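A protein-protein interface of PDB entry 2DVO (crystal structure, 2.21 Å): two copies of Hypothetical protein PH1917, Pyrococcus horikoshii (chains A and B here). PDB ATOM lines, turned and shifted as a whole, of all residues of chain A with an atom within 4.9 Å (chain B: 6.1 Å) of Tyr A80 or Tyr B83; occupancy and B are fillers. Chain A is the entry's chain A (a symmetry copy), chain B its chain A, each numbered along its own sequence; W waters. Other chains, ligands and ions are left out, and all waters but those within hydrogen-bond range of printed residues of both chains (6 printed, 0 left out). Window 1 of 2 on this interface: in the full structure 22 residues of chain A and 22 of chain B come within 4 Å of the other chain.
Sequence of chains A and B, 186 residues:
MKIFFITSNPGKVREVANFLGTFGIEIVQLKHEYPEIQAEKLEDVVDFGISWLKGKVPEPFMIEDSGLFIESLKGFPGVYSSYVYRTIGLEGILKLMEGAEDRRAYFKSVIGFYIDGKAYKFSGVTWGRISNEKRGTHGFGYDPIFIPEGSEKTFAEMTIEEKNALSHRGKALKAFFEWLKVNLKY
OH of Tyr B83 lies within hydrogen-bond range of O of Gly A75 (3.4 Å). N of Phe A76 lies close to OH of Tyr B83. NH2 of Arg B86 is in salt-bridge range of OE2 of Glu A40 (3.4 Å).
The backbone carbonyl oxygen (O) of Tyr B83 is in hydrogen-bond range of the side-chain hydroxyl (OG1) of Thr B87, at 3.0 Å. The backbone carbonyl oxygen (O) of Val B84 is in hydrogen-bond range of the side-chain hydroxyl (OG1) of Thr B87, at 3.3 Å. The backbone NH (N) of Ala A39 is in hydrogen-bond range of the side-chain hydroxyl (OH) of Tyr A80 (3.0 Å). The backbone carbonyl oxygen (O) of Gly A78 lies within hydrogen-bond range of the side-chain hydroxyl (OG) of Ser A81, 2.5 Å away.
Among the printed residues, pairs that only touch across the chains: Gln A38 with Gln B38 (3.9 Å), Gln A38 with Tyr B80 (3.9 Å), Glu A40 with Tyr B83 (3.8 Å), Lys A74 with Thr B87 (3.4 Å), Phe A76 with Thr B87 (3.6 Å), Phe A76 with Ile B88 (3.9 Å), Pro A77 with Tyr B83 (3.5 Å), Gly A78 with Tyr B83 (3.8 Å), Val A79 with Gln B38 (3.97 Å), Tyr A80 with Gln B38 (3.9 Å), Tyr A80 with Tyr B80 (3.6 Å), Tyr A80 with Tyr B83 (3.3 Å) and Tyr A83 with Tyr B80 (3.3 Å).
Tyr A80 touches just these residues of chain B: Gln B38, Tyr B80 and Tyr B83. Of the printed residues of chain A, Tyr B80 touches Gln A38, Tyr A80 and Tyr A83. Of the printed residues of chain B, Gly A75 touches Tyr B83 (3.4 Å). Printed residues of chain A within 4 Å of Thr B87: Lys A74 and Phe A76. Tyr B85 touches none of the printed residues of chain A. The nearest residue of chain A that does not touch Tyr B83 is Val A79 (4.8 Å). The nearest printed residue of chain B that does not touch Pro A77 is Thr B87 (6.4 Å).
Printed residues of chain B that touch a printed residue of chain A: Gln B38, Tyr B80, Tyr B83, Arg B86, Thr B87 and Ile B88. Hydrophobic or aromatic side chains of chain B that line the printed part of chain A: Tyr B80, Tyr B83 and Ile B88. Printed residues of chain A that touch a printed residue of chain B: Gln A38, Glu A40, Lys A74, Gly A75, Phe A76, Pro A77, Gly A78, Val A79, Tyr A80 and Tyr A83. Among the printed residues, 16 pairs touch across the chains.
Gln A38 touches its own counterpart, Gln B38. Gln A38 touches Tyr B80, and with the chains exchanged Tyr A80 touches Gln B38. Tyr A80 touches its own counterpart, Tyr B80. Tyr A80 touches Tyr B83, and with the chains exchanged Tyr A83 touches Tyr B80. Positions printed for both chains: 38, 80, 81, 82, 83 and 84. Of the 16 pairs that touch across the chains among the printed residues, 6 have their exchanged pair printed and touching as well.
Water W6 lies within hydrogen-bond range of NZ of Lys A74 (2.7 Å) and O of Thr B87 (3.1 Å). Water W2 bridges the backbone carbonyl oxygen (O) of Val A79 and the side-chain amide nitrogen (NE2) of Gln B38. Water W1 lies within hydrogen-bond range of O of Lys A74 (2.8 Å) and OH of Tyr B83 (2.8 Å). Water W4 bridges N of Val A79 (3.0 Å) and OH of Tyr B83 (3.3 Å). Water W5 bridges N of Tyr A83 (3.2 Å) and OE1 of Gln B38 (3.4 Å). Water W3 bridges the backbone NH (N) of Tyr B83 and the side-chain amide oxygen (OE1) of Gln A38.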
ATOM      1  N   GLN A  38     -18.748   0.185 -32.642  1.00  0.00           N
ATOM      2  CA  GLN A  38     -17.336   0.349 -32.356  1.00  0.00           C
ATOM      3  C   GLN A  38     -16.542  -0.802 -32.972  1.00  0.00           C
ATOM      4  O   GLN A  38     -16.922  -1.964 -32.903  1.00  0.00           O
ATOM      5  CB  GLN A  38     -17.157   0.367 -30.832  1.00  0.00           C
ATOM      6  CG  GLN A  38     -17.822   1.581 -30.183  1.00  0.00           C
ATOM      7  CD  GLN A  38     -17.814   1.422 -28.681  1.00  0.00           C
ATOM      8  OE1 GLN A  38     -16.812   1.119 -28.056  1.00  0.00           O
ATOM      9  NE2 GLN A  38     -18.997   1.684 -28.095  1.00  0.00           N
ATOM     10  N   ALA A  39     -15.419  -0.527 -33.621  1.00  0.00           N
ATOM     11  CA  ALA A  39     -14.638  -1.588 -34.241  1.00  0.00           C
ATOM     12  C   ALA A  39     -13.255  -1.065 -34.583  1.00  0.00           C
ATOM     13  O   ALA A  39     -12.996   0.135 -34.502  1.00  0.00           O
ATOM     14  CB  ALA A  39     -15.342  -2.085 -35.508  1.00  0.00           C
ATOM     15  N   GLU A  40     -12.368  -1.972 -34.961  1.00  0.00           N
ATOM     16  CA  GLU A  40     -11.002  -1.594 -35.305  1.00  0.00           C
ATOM     17  C   GLU A  40     -10.868  -1.277 -36.785  1.00  0.00           C
ATOM     18  O   GLU A  40      -9.929  -0.609 -37.199  1.00  0.00           O
ATOM     19  CB  GLU A  40     -10.034  -2.716 -34.911  1.00  0.00           C
ATOM     20  CG  GLU A  40      -9.817  -2.829 -33.400  1.00  0.00           C
ATOM     21  CD  GLU A  40      -9.051  -1.640 -32.830  1.00  0.00           C
ATOM     22  OE1 GLU A  40      -7.835  -1.532 -33.102  1.00  0.00           O
ATOM     23  OE2 GLU A  40      -9.661  -0.813 -32.119  1.00  0.00           O
ATOM     24  N   LYS A  74      -0.775   6.271 -33.162  1.00  0.00           N
ATOM     25  CA  LYS A  74      -1.158   4.874 -33.342  1.00  0.00           C
ATOM     26  C   LYS A  74      -2.478   4.653 -34.094  1.00  0.00           C
ATOM     27  O   LYS A  74      -3.197   3.694 -33.817  1.00  0.00           O
ATOM     28  CB  LYS A  74      -1.218   4.161 -31.982  1.00  0.00           C
ATOM     29  CG  LYS A  74       0.105   4.139 -31.210  1.00  0.00           C
ATOM     30  CD  LYS A  74      -0.001   3.222 -29.998  1.00  0.00           C
ATOM     31  CE  LYS A  74       1.324   3.086 -29.258  1.00  0.00           C
ATOM     32  NZ  LYS A  74       1.785   4.374 -28.670  1.00  0.00           N
ATOM     33  N   GLY A  75      -2.789   5.526 -35.054  1.00  0.00           N
ATOM     34  CA  GLY A  75      -4.013   5.361 -35.825  1.00  0.00           C
ATOM     35  C   GLY A  75      -5.154   6.274 -35.410  1.00  0.00           C
ATOM     36  O   GLY A  75      -6.096   6.504 -36.166  1.00  0.00           O
ATOM     37  N   PHE A  76      -5.067   6.788 -34.192  1.00  0.00           N
ATOM     38  CA  PHE A  76      -6.067   7.692 -33.646  1.00  0.00           C
ATOM     39  C   PHE A  76      -6.164   8.903 -34.576  1.00  0.00           C
ATOM     40  O   PHE A  76      -5.162   9.324 -35.148  1.00  0.00           O
ATOM     41  CB  PHE A  76      -5.616   8.095 -32.235  1.00  0.00           C
ATOM     42  CG  PHE A  76      -6.397   9.224 -31.621  1.00  0.00           C
ATOM     43  CD1 PHE A  76      -6.168  10.539 -32.007  1.00  0.00           C
ATOM     44  CD2 PHE A  76      -7.309   8.974 -30.600  1.00  0.00           C
ATOM     45  CE1 PHE A  76      -6.835  11.594 -31.381  1.00  0.00           C
ATOM     46  CE2 PHE A  76      -7.977  10.019 -29.969  1.00  0.00           C
ATOM     47  CZ  PHE A  76      -7.739  11.332 -30.358  1.00  0.00           C
ATOM     48  N   PRO A  77      -7.370   9.479 -34.743  1.00  0.00           N
ATOM     49  CA  PRO A  77      -8.645   9.088 -34.129  1.00  0.00           C
ATOM     50  C   PRO A  77      -9.384   7.983 -34.881  1.00  0.00           C
ATOM     51  O   PRO A  77     -10.377   7.461 -34.389  1.00  0.00           O
ATOM     52  CB  PRO A  77      -9.419  10.398 -34.097  1.00  0.00           C
ATOM     53  CG  PRO A  77      -8.984  11.055 -35.384  1.00  0.00           C
ATOM     54  CD  PRO A  77      -7.493  10.782 -35.425  1.00  0.00           C
ATOM     55  N   GLY A  78      -8.894   7.652 -36.077  1.00  0.00           N
ATOM     56  CA  GLY A  78      -9.472   6.589 -36.891  1.00  0.00           C
ATOM     57  C   GLY A  78     -10.982   6.488 -37.019  1.00  0.00           C
ATOM     58  O   GLY A  78     -11.651   7.434 -37.417  1.00  0.00           O
ATOM     59  N   VAL A  79     -11.504   5.311 -36.696  1.00  0.00           N
ATOM     60  CA  VAL A  79     -12.932   5.021 -36.784  1.00  0.00           C
ATOM     61  C   VAL A  79     -13.778   6.022 -35.989  1.00  0.00           C
ATOM     62  O   VAL A  79     -14.940   6.273 -36.284  1.00  0.00           O
ATOM     63  CB  VAL A  79     -13.163   3.605 -36.254  1.00  0.00           C
ATOM     64  CG1 VAL A  79     -14.660   3.310 -36.190  1.00  0.00           C
ATOM     65  CG2 VAL A  79     -12.494   2.594 -37.167  1.00  0.00           C
ATOM     66  N   TYR A  80     -13.170   6.575 -34.922  1.00  0.00           N
ATOM     67  CA  TYR A  80     -13.914   7.508 -34.077  1.00  0.00           C
ATOM     68  C   TYR A  80     -13.519   8.963 -34.340  1.00  0.00           C
ATOM     69  O   TYR A  80     -13.574   9.818 -33.465  1.00  0.00           O
ATOM     70  CB  TYR A  80     -13.643   7.151 -32.615  1.00  0.00           C
ATOM     71  CG  TYR A  80     -13.856   5.695 -32.402  1.00  0.00           C
ATOM     72  CD1 TYR A  80     -15.148   5.177 -32.402  1.00  0.00           C
ATOM     73  CD2 TYR A  80     -12.770   4.843 -32.198  1.00  0.00           C
ATOM     74  CE1 TYR A  80     -15.353   3.817 -32.212  1.00  0.00           C
ATOM     75  CE2 TYR A  80     -12.975   3.488 -31.998  1.00  0.00           C
ATOM     76  CZ  TYR A  80     -14.259   2.974 -32.000  1.00  0.00           C
ATOM     77  OH  TYR A  80     -14.470   1.621 -31.817  1.00  0.00           O
ATOM     78  N   SER A  81     -13.183   9.235 -35.598  1.00  0.00           N
ATOM     79  CA  SER A  81     -12.828  10.583 -36.033  1.00  0.00           C
ATOM     80  C   SER A  81     -13.926  11.614 -35.769  1.00  0.00           C
ATOM     81  O   SER A  81     -13.644  12.753 -35.394  1.00  0.00           O
ATOM     82  CB  SER A  81     -12.479  10.579 -37.525  1.00  0.00           C
ATOM     83  OG  SER A  81     -11.272   9.876 -37.756  1.00  0.00           O
ATOM     84  N   SER A  82     -15.177  11.215 -35.965  1.00  0.00           N
ATOM     85  CA  SER A  82     -16.297  12.127 -35.752  1.00  0.00           C
ATOM     86  C   SER A  82     -16.399  12.601 -34.303  1.00  0.00           C
ATOM     87  O   SER A  82     -16.462  13.804 -34.036  1.00  0.00           O
ATOM     88  CB  SER A  82     -17.608  11.460 -36.164  1.00  0.00           C
ATOM     89  OG  SER A  82     -18.693  12.353 -35.990  1.00  0.00           O
ATOM     90  N   TYR A  83     -16.422  11.658 -33.369  1.00  0.00           N
ATOM     91  CA  TYR A  83     -16.510  12.006 -31.956  1.00  0.00           C
ATOM     92  C   TYR A  83     -15.338  12.869 -31.511  1.00  0.00           C
ATOM     93  O   TYR A  83     -15.522  13.856 -30.792  1.00  0.00           O
ATOM     94  CB  TYR A  83     -16.547  10.746 -31.101  1.00  0.00           C
ATOM     95  CG  TYR A  83     -16.514  11.035 -29.621  1.00  0.00           C
ATOM     96  CD1 TYR A  83     -17.638  11.533 -28.961  1.00  0.00           C
ATOM     97  CD2 TYR A  83     -15.348  10.828 -28.880  1.00  0.00           C
ATOM     98  CE1 TYR A  83     -17.602  11.818 -27.593  1.00  0.00           C
ATOM     99  CE2 TYR A  83     -15.300  11.110 -27.519  1.00  0.00           C
ATOM    100  CZ  TYR A  83     -16.427  11.603 -26.880  1.00  0.00           C
ATOM    101  OH  TYR A  83     -16.375  11.874 -25.528  1.00  0.00           O
ATOM    102  N   VAL A  84     -14.130  12.481 -31.918  1.00  0.00           N
ATOM    103  CA  VAL A  84     -12.930  13.222 -31.554  1.00  0.00           C
ATOM    104  C   VAL A  84     -12.961  14.634 -32.116  1.00  0.00           C
ATOM    105  O   VAL A  84     -12.484  15.573 -31.480  1.00  0.00           O
ATOM    106  CB  VAL A  84     -11.659  12.515 -32.061  1.00  0.00           C
ATOM    107  CG1 VAL A  84     -10.434  13.378 -31.787  1.00  0.00           C
ATOM    108  CG2 VAL A  84     -11.520  11.163 -31.384  1.00  0.00           C
ATOM    109  N   GLN B  38     -21.406   2.820 -31.474  1.00  0.00           N
ATOM    110  CA  GLN B  38     -21.046   4.199 -31.207  1.00  0.00           C
ATOM    111  C   GLN B  38     -22.270   4.975 -30.726  1.00  0.00           C
ATOM    112  O   GLN B  38     -23.368   4.852 -31.254  1.00  0.00           O
ATOM    113  CB  GLN B  38     -20.503   4.810 -32.505  1.00  0.00           C
ATOM    114  CG  GLN B  38     -19.197   4.153 -32.955  1.00  0.00           C
ATOM    115  CD  GLN B  38     -18.840   4.630 -34.344  1.00  0.00           C
ATOM    116  OE1 GLN B  38     -18.836   5.809 -34.655  1.00  0.00           O
ATOM    117  NE2 GLN B  38     -18.491   3.643 -35.189  1.00  0.00           N
ATOM    118  N   TYR B  80     -15.738   6.218 -25.687  1.00  0.00           N
ATOM    119  CA  TYR B  80     -14.638   5.596 -26.420  1.00  0.00           C
ATOM    120  C   TYR B  80     -13.329   5.623 -25.626  1.00  0.00           C
ATOM    121  O   TYR B  80     -12.238   5.672 -26.178  1.00  0.00           O
ATOM    122  CB  TYR B  80     -14.460   6.344 -27.742  1.00  0.00           C
ATOM    123  CG  TYR B  80     -15.771   6.473 -28.431  1.00  0.00           C
ATOM    124  CD1 TYR B  80     -16.359   5.356 -29.017  1.00  0.00           C
ATOM    125  CD2 TYR B  80     -16.417   7.708 -28.497  1.00  0.00           C
ATOM    126  CE1 TYR B  80     -17.587   5.468 -29.654  1.00  0.00           C
ATOM    127  CE2 TYR B  80     -17.638   7.823 -29.143  1.00  0.00           C
ATOM    128  CZ  TYR B  80     -18.221   6.711 -29.723  1.00  0.00           C
ATOM    129  OH  TYR B  80     -19.445   6.814 -30.354  1.00  0.00           O
ATOM    130  N   SER B  81     -13.471   5.520 -24.308  1.00  0.00           N
ATOM    131  CA  SER B  81     -12.324   5.480 -23.404  1.00  0.00           C
ATOM    132  C   SER B  81     -11.354   4.337 -23.708  1.00  0.00           C
ATOM    133  O   SER B  81     -10.136   4.503 -23.616  1.00  0.00           O
ATOM    134  CB  SER B  81     -12.802   5.371 -21.953  1.00  0.00           C
ATOM    135  OG  SER B  81     -13.446   6.566 -21.546  1.00  0.00           O
ATOM    136  N   SER B  82     -11.892   3.179 -24.071  1.00  0.00           N
ATOM    137  CA  SER B  82     -11.052   2.023 -24.371  1.00  0.00           C
ATOM    138  C   SER B  82     -10.129   2.264 -25.564  1.00  0.00           C
ATOM    139  O   SER B  82      -8.915   2.063 -25.471  1.00  0.00           O
ATOM    140  CB  SER B  82     -11.921   0.795 -24.638  1.00  0.00           C
ATOM    141  OG  SER B  82     -11.109  -0.336 -24.897  1.00  0.00           O
ATOM    142  N   TYR B  83     -10.701   2.689 -26.683  1.00  0.00           N
ATOM    143  CA  TYR B  83      -9.906   2.956 -27.876  1.00  0.00           C
ATOM    144  C   TYR B  83      -8.855   4.028 -27.628  1.00  0.00           C
ATOM    145  O   TYR B  83      -7.701   3.885 -28.045  1.00  0.00           O
ATOM    146  CB  TYR B  83     -10.804   3.403 -29.023  1.00  0.00           C
ATOM    147  CG  TYR B  83     -10.033   3.814 -30.252  1.00  0.00           C
ATOM    148  CD1 TYR B  83      -9.432   2.861 -31.074  1.00  0.00           C
ATOM    149  CD2 TYR B  83      -9.886   5.163 -30.583  1.00  0.00           C
ATOM    150  CE1 TYR B  83      -8.701   3.243 -32.204  1.00  0.00           C
ATOM    151  CE2 TYR B  83      -9.160   5.554 -31.703  1.00  0.00           C
ATOM    152  CZ  TYR B  83      -8.571   4.594 -32.510  1.00  0.00           C
ATOM    153  OH  TYR B  83      -7.857   4.988 -33.623  1.00  0.00           O
ATOM    154  N   VAL B  84      -9.261   5.114 -26.970  1.00  0.00           N
ATOM    155  CA  VAL B  84      -8.349   6.211 -26.676  1.00  0.00           C
ATOM    156  C   VAL B  84      -7.215   5.758 -25.770  1.00  0.00           C
ATOM    157  O   VAL B  84      -6.084   6.222 -25.905  1.00  0.00           O
ATOM    158  CB  VAL B  84      -9.084   7.385 -26.002  1.00  0.00           C
ATOM    159  CG1 VAL B  84      -8.086   8.458 -25.583  1.00  0.00           C
ATOM    160  CG2 VAL B  84     -10.113   7.961 -26.956  1.00  0.00           C
ATOM    161  N   TYR B  85      -7.512   4.851 -24.848  1.00  0.00           N
ATOM    162  CA  TYR B  85      -6.490   4.360 -23.938  1.00  0.00           C
ATOM    163  C   TYR B  85      -5.455   3.565 -24.716  1.00  0.00           C
ATOM    164  O   TYR B  85      -4.247   3.699 -24.494  1.00  0.00           O
ATOM    165  CB  TYR B  85      -7.095   3.444 -22.872  1.00  0.00           C
ATOM    166  CG  TYR B  85      -6.038   2.796 -22.013  1.00  0.00           C
ATOM    167  CD1 TYR B  85      -5.366   3.527 -21.029  1.00  0.00           C
ATOM    168  CD2 TYR B  85      -5.669   1.467 -22.215  1.00  0.00           C
ATOM    169  CE1 TYR B  85      -4.349   2.946 -20.265  1.00  0.00           C
ATOM    170  CE2 TYR B  85      -4.653   0.875 -21.459  1.00  0.00           C
ATOM    171  CZ  TYR B  85      -3.999   1.619 -20.487  1.00  0.00           C
ATOM    172  OH  TYR B  85      -2.999   1.036 -19.743  1.00  0.00           O
ATOM    173  N   ARG B  86      -5.944   2.729 -25.628  1.00  0.00           N
ATOM    174  CA  ARG B  86      -5.067   1.886 -26.431  1.00  0.00           C
ATOM    175  C   ARG B  86      -4.285   2.627 -27.498  1.00  0.00           C
ATOM    176  O   ARG B  86      -3.297   2.100 -28.008  1.00  0.00           O
ATOM    177  CB  ARG B  86      -5.857   0.740 -27.077  1.00  0.00           C
ATOM    178  CG  ARG B  86      -6.199  -0.363 -26.092  1.00  0.00           C
ATOM    179  CD  ARG B  86      -6.944  -1.512 -26.735  1.00  0.00           C
ATOM    180  NE  ARG B  86      -8.279  -1.132 -27.183  1.00  0.00           N
ATOM    181  CZ  ARG B  86      -8.600  -0.871 -28.446  1.00  0.00           C
ATOM    182  NH1 ARG B  86      -7.680  -0.944 -29.397  1.00  0.00           N
ATOM    183  NH2 ARG B  86      -9.850  -0.554 -28.766  1.00  0.00           N
ATOM    184  N   THR B  87      -4.709   3.839 -27.840  1.00  0.00           N
ATOM    185  CA  THR B  87      -3.985   4.592 -28.847  1.00  0.00           C
ATOM    186  C   THR B  87      -3.073   5.665 -28.253  1.00  0.00           C
ATOM    187  O   THR B  87      -1.861   5.466 -28.193  1.00  0.00           O
ATOM    188  CB  THR B  87      -4.939   5.205 -29.888  1.00  0.00           C
ATOM    189  OG1 THR B  87      -5.941   5.988 -29.233  1.00  0.00           O
ATOM    190  CG2 THR B  87      -5.614   4.094 -30.687  1.00  0.00           C
ATOM    191  N   ILE B  88      -3.623   6.788 -27.808  1.00  0.00           N
ATOM    192  CA  ILE B  88      -2.776   7.828 -27.240  1.00  0.00           C
ATOM    193  C   ILE B  88      -2.394   7.536 -25.784  1.00  0.00           C
ATOM    194  O   ILE B  88      -1.432   8.102 -25.261  1.00  0.00           O
ATOM    195  CB  ILE B  88      -3.449   9.213 -27.339  1.00  0.00           C
ATOM    196  CG1 ILE B  88      -4.722   9.255 -26.492  1.00  0.00           C
ATOM    197  CG2 ILE B  88      -3.761   9.522 -28.798  1.00  0.00           C
ATOM    198  CD1 ILE B  88      -5.395  10.610 -26.499  1.00  0.00           C
ATOM    199  N   GLY B  89      -3.145   6.647 -25.140  1.00  0.00           N
ATOM    200  CA  GLY B  89      -2.861   6.283 -23.763  1.00  0.00           C
ATOM    201  C   GLY B  89      -2.879   7.402 -22.735  1.00  0.00           C
ATOM    202  O   GLY B  89      -3.325   8.520 -23.002  1.00  0.00           O
ATOM    203  N   TYR B 142      -7.261   4.088 -16.967  1.00  0.00           N
ATOM    204  CA  TYR B 142      -6.953   5.445 -16.524  1.00  0.00           C
ATOM    205  C   TYR B 142      -6.746   5.620 -15.018  1.00  0.00           C
ATOM    206  O   TYR B 142      -6.564   6.742 -14.548  1.00  0.00           O
ATOM    207  CB  TYR B 142      -8.064   6.394 -16.985  1.00  0.00           C
ATOM    208  CG  TYR B 142      -8.249   6.451 -18.487  1.00  0.00           C
ATOM    209  CD1 TYR B 142      -7.503   7.327 -19.266  1.00  0.00           C
ATOM    210  CD2 TYR B 142      -9.168   5.622 -19.125  1.00  0.00           C
ATOM    211  CE1 TYR B 142      -7.666   7.382 -20.639  1.00  0.00           C
ATOM    212  CE2 TYR B 142      -9.338   5.667 -20.508  1.00  0.00           C
ATOM    213  CZ  TYR B 142      -8.584   6.551 -21.256  1.00  0.00           C
ATOM    214  OH  TYR B 142      -8.733   6.597 -22.628  1.00  0.00           O
HETATM  215  O   HOH W   1      -5.894   3.075 -34.339  1.00  0.00           O
HETATM  216  O   HOH W   2     -17.165   5.122 -37.484  1.00  0.00           O
HETATM  217  O   HOH W   3     -13.820   2.469 -27.281  1.00  0.00           O
HETATM  218  O   HOH W   4      -9.846   3.146 -35.543  1.00  0.00           O
HETATM  219  O   HOH W   5     -17.074   8.596 -33.947  1.00  0.00           O
HETATM  220  O   HOH W   6       0.326   4.213 -26.424  1.00  0.00           O
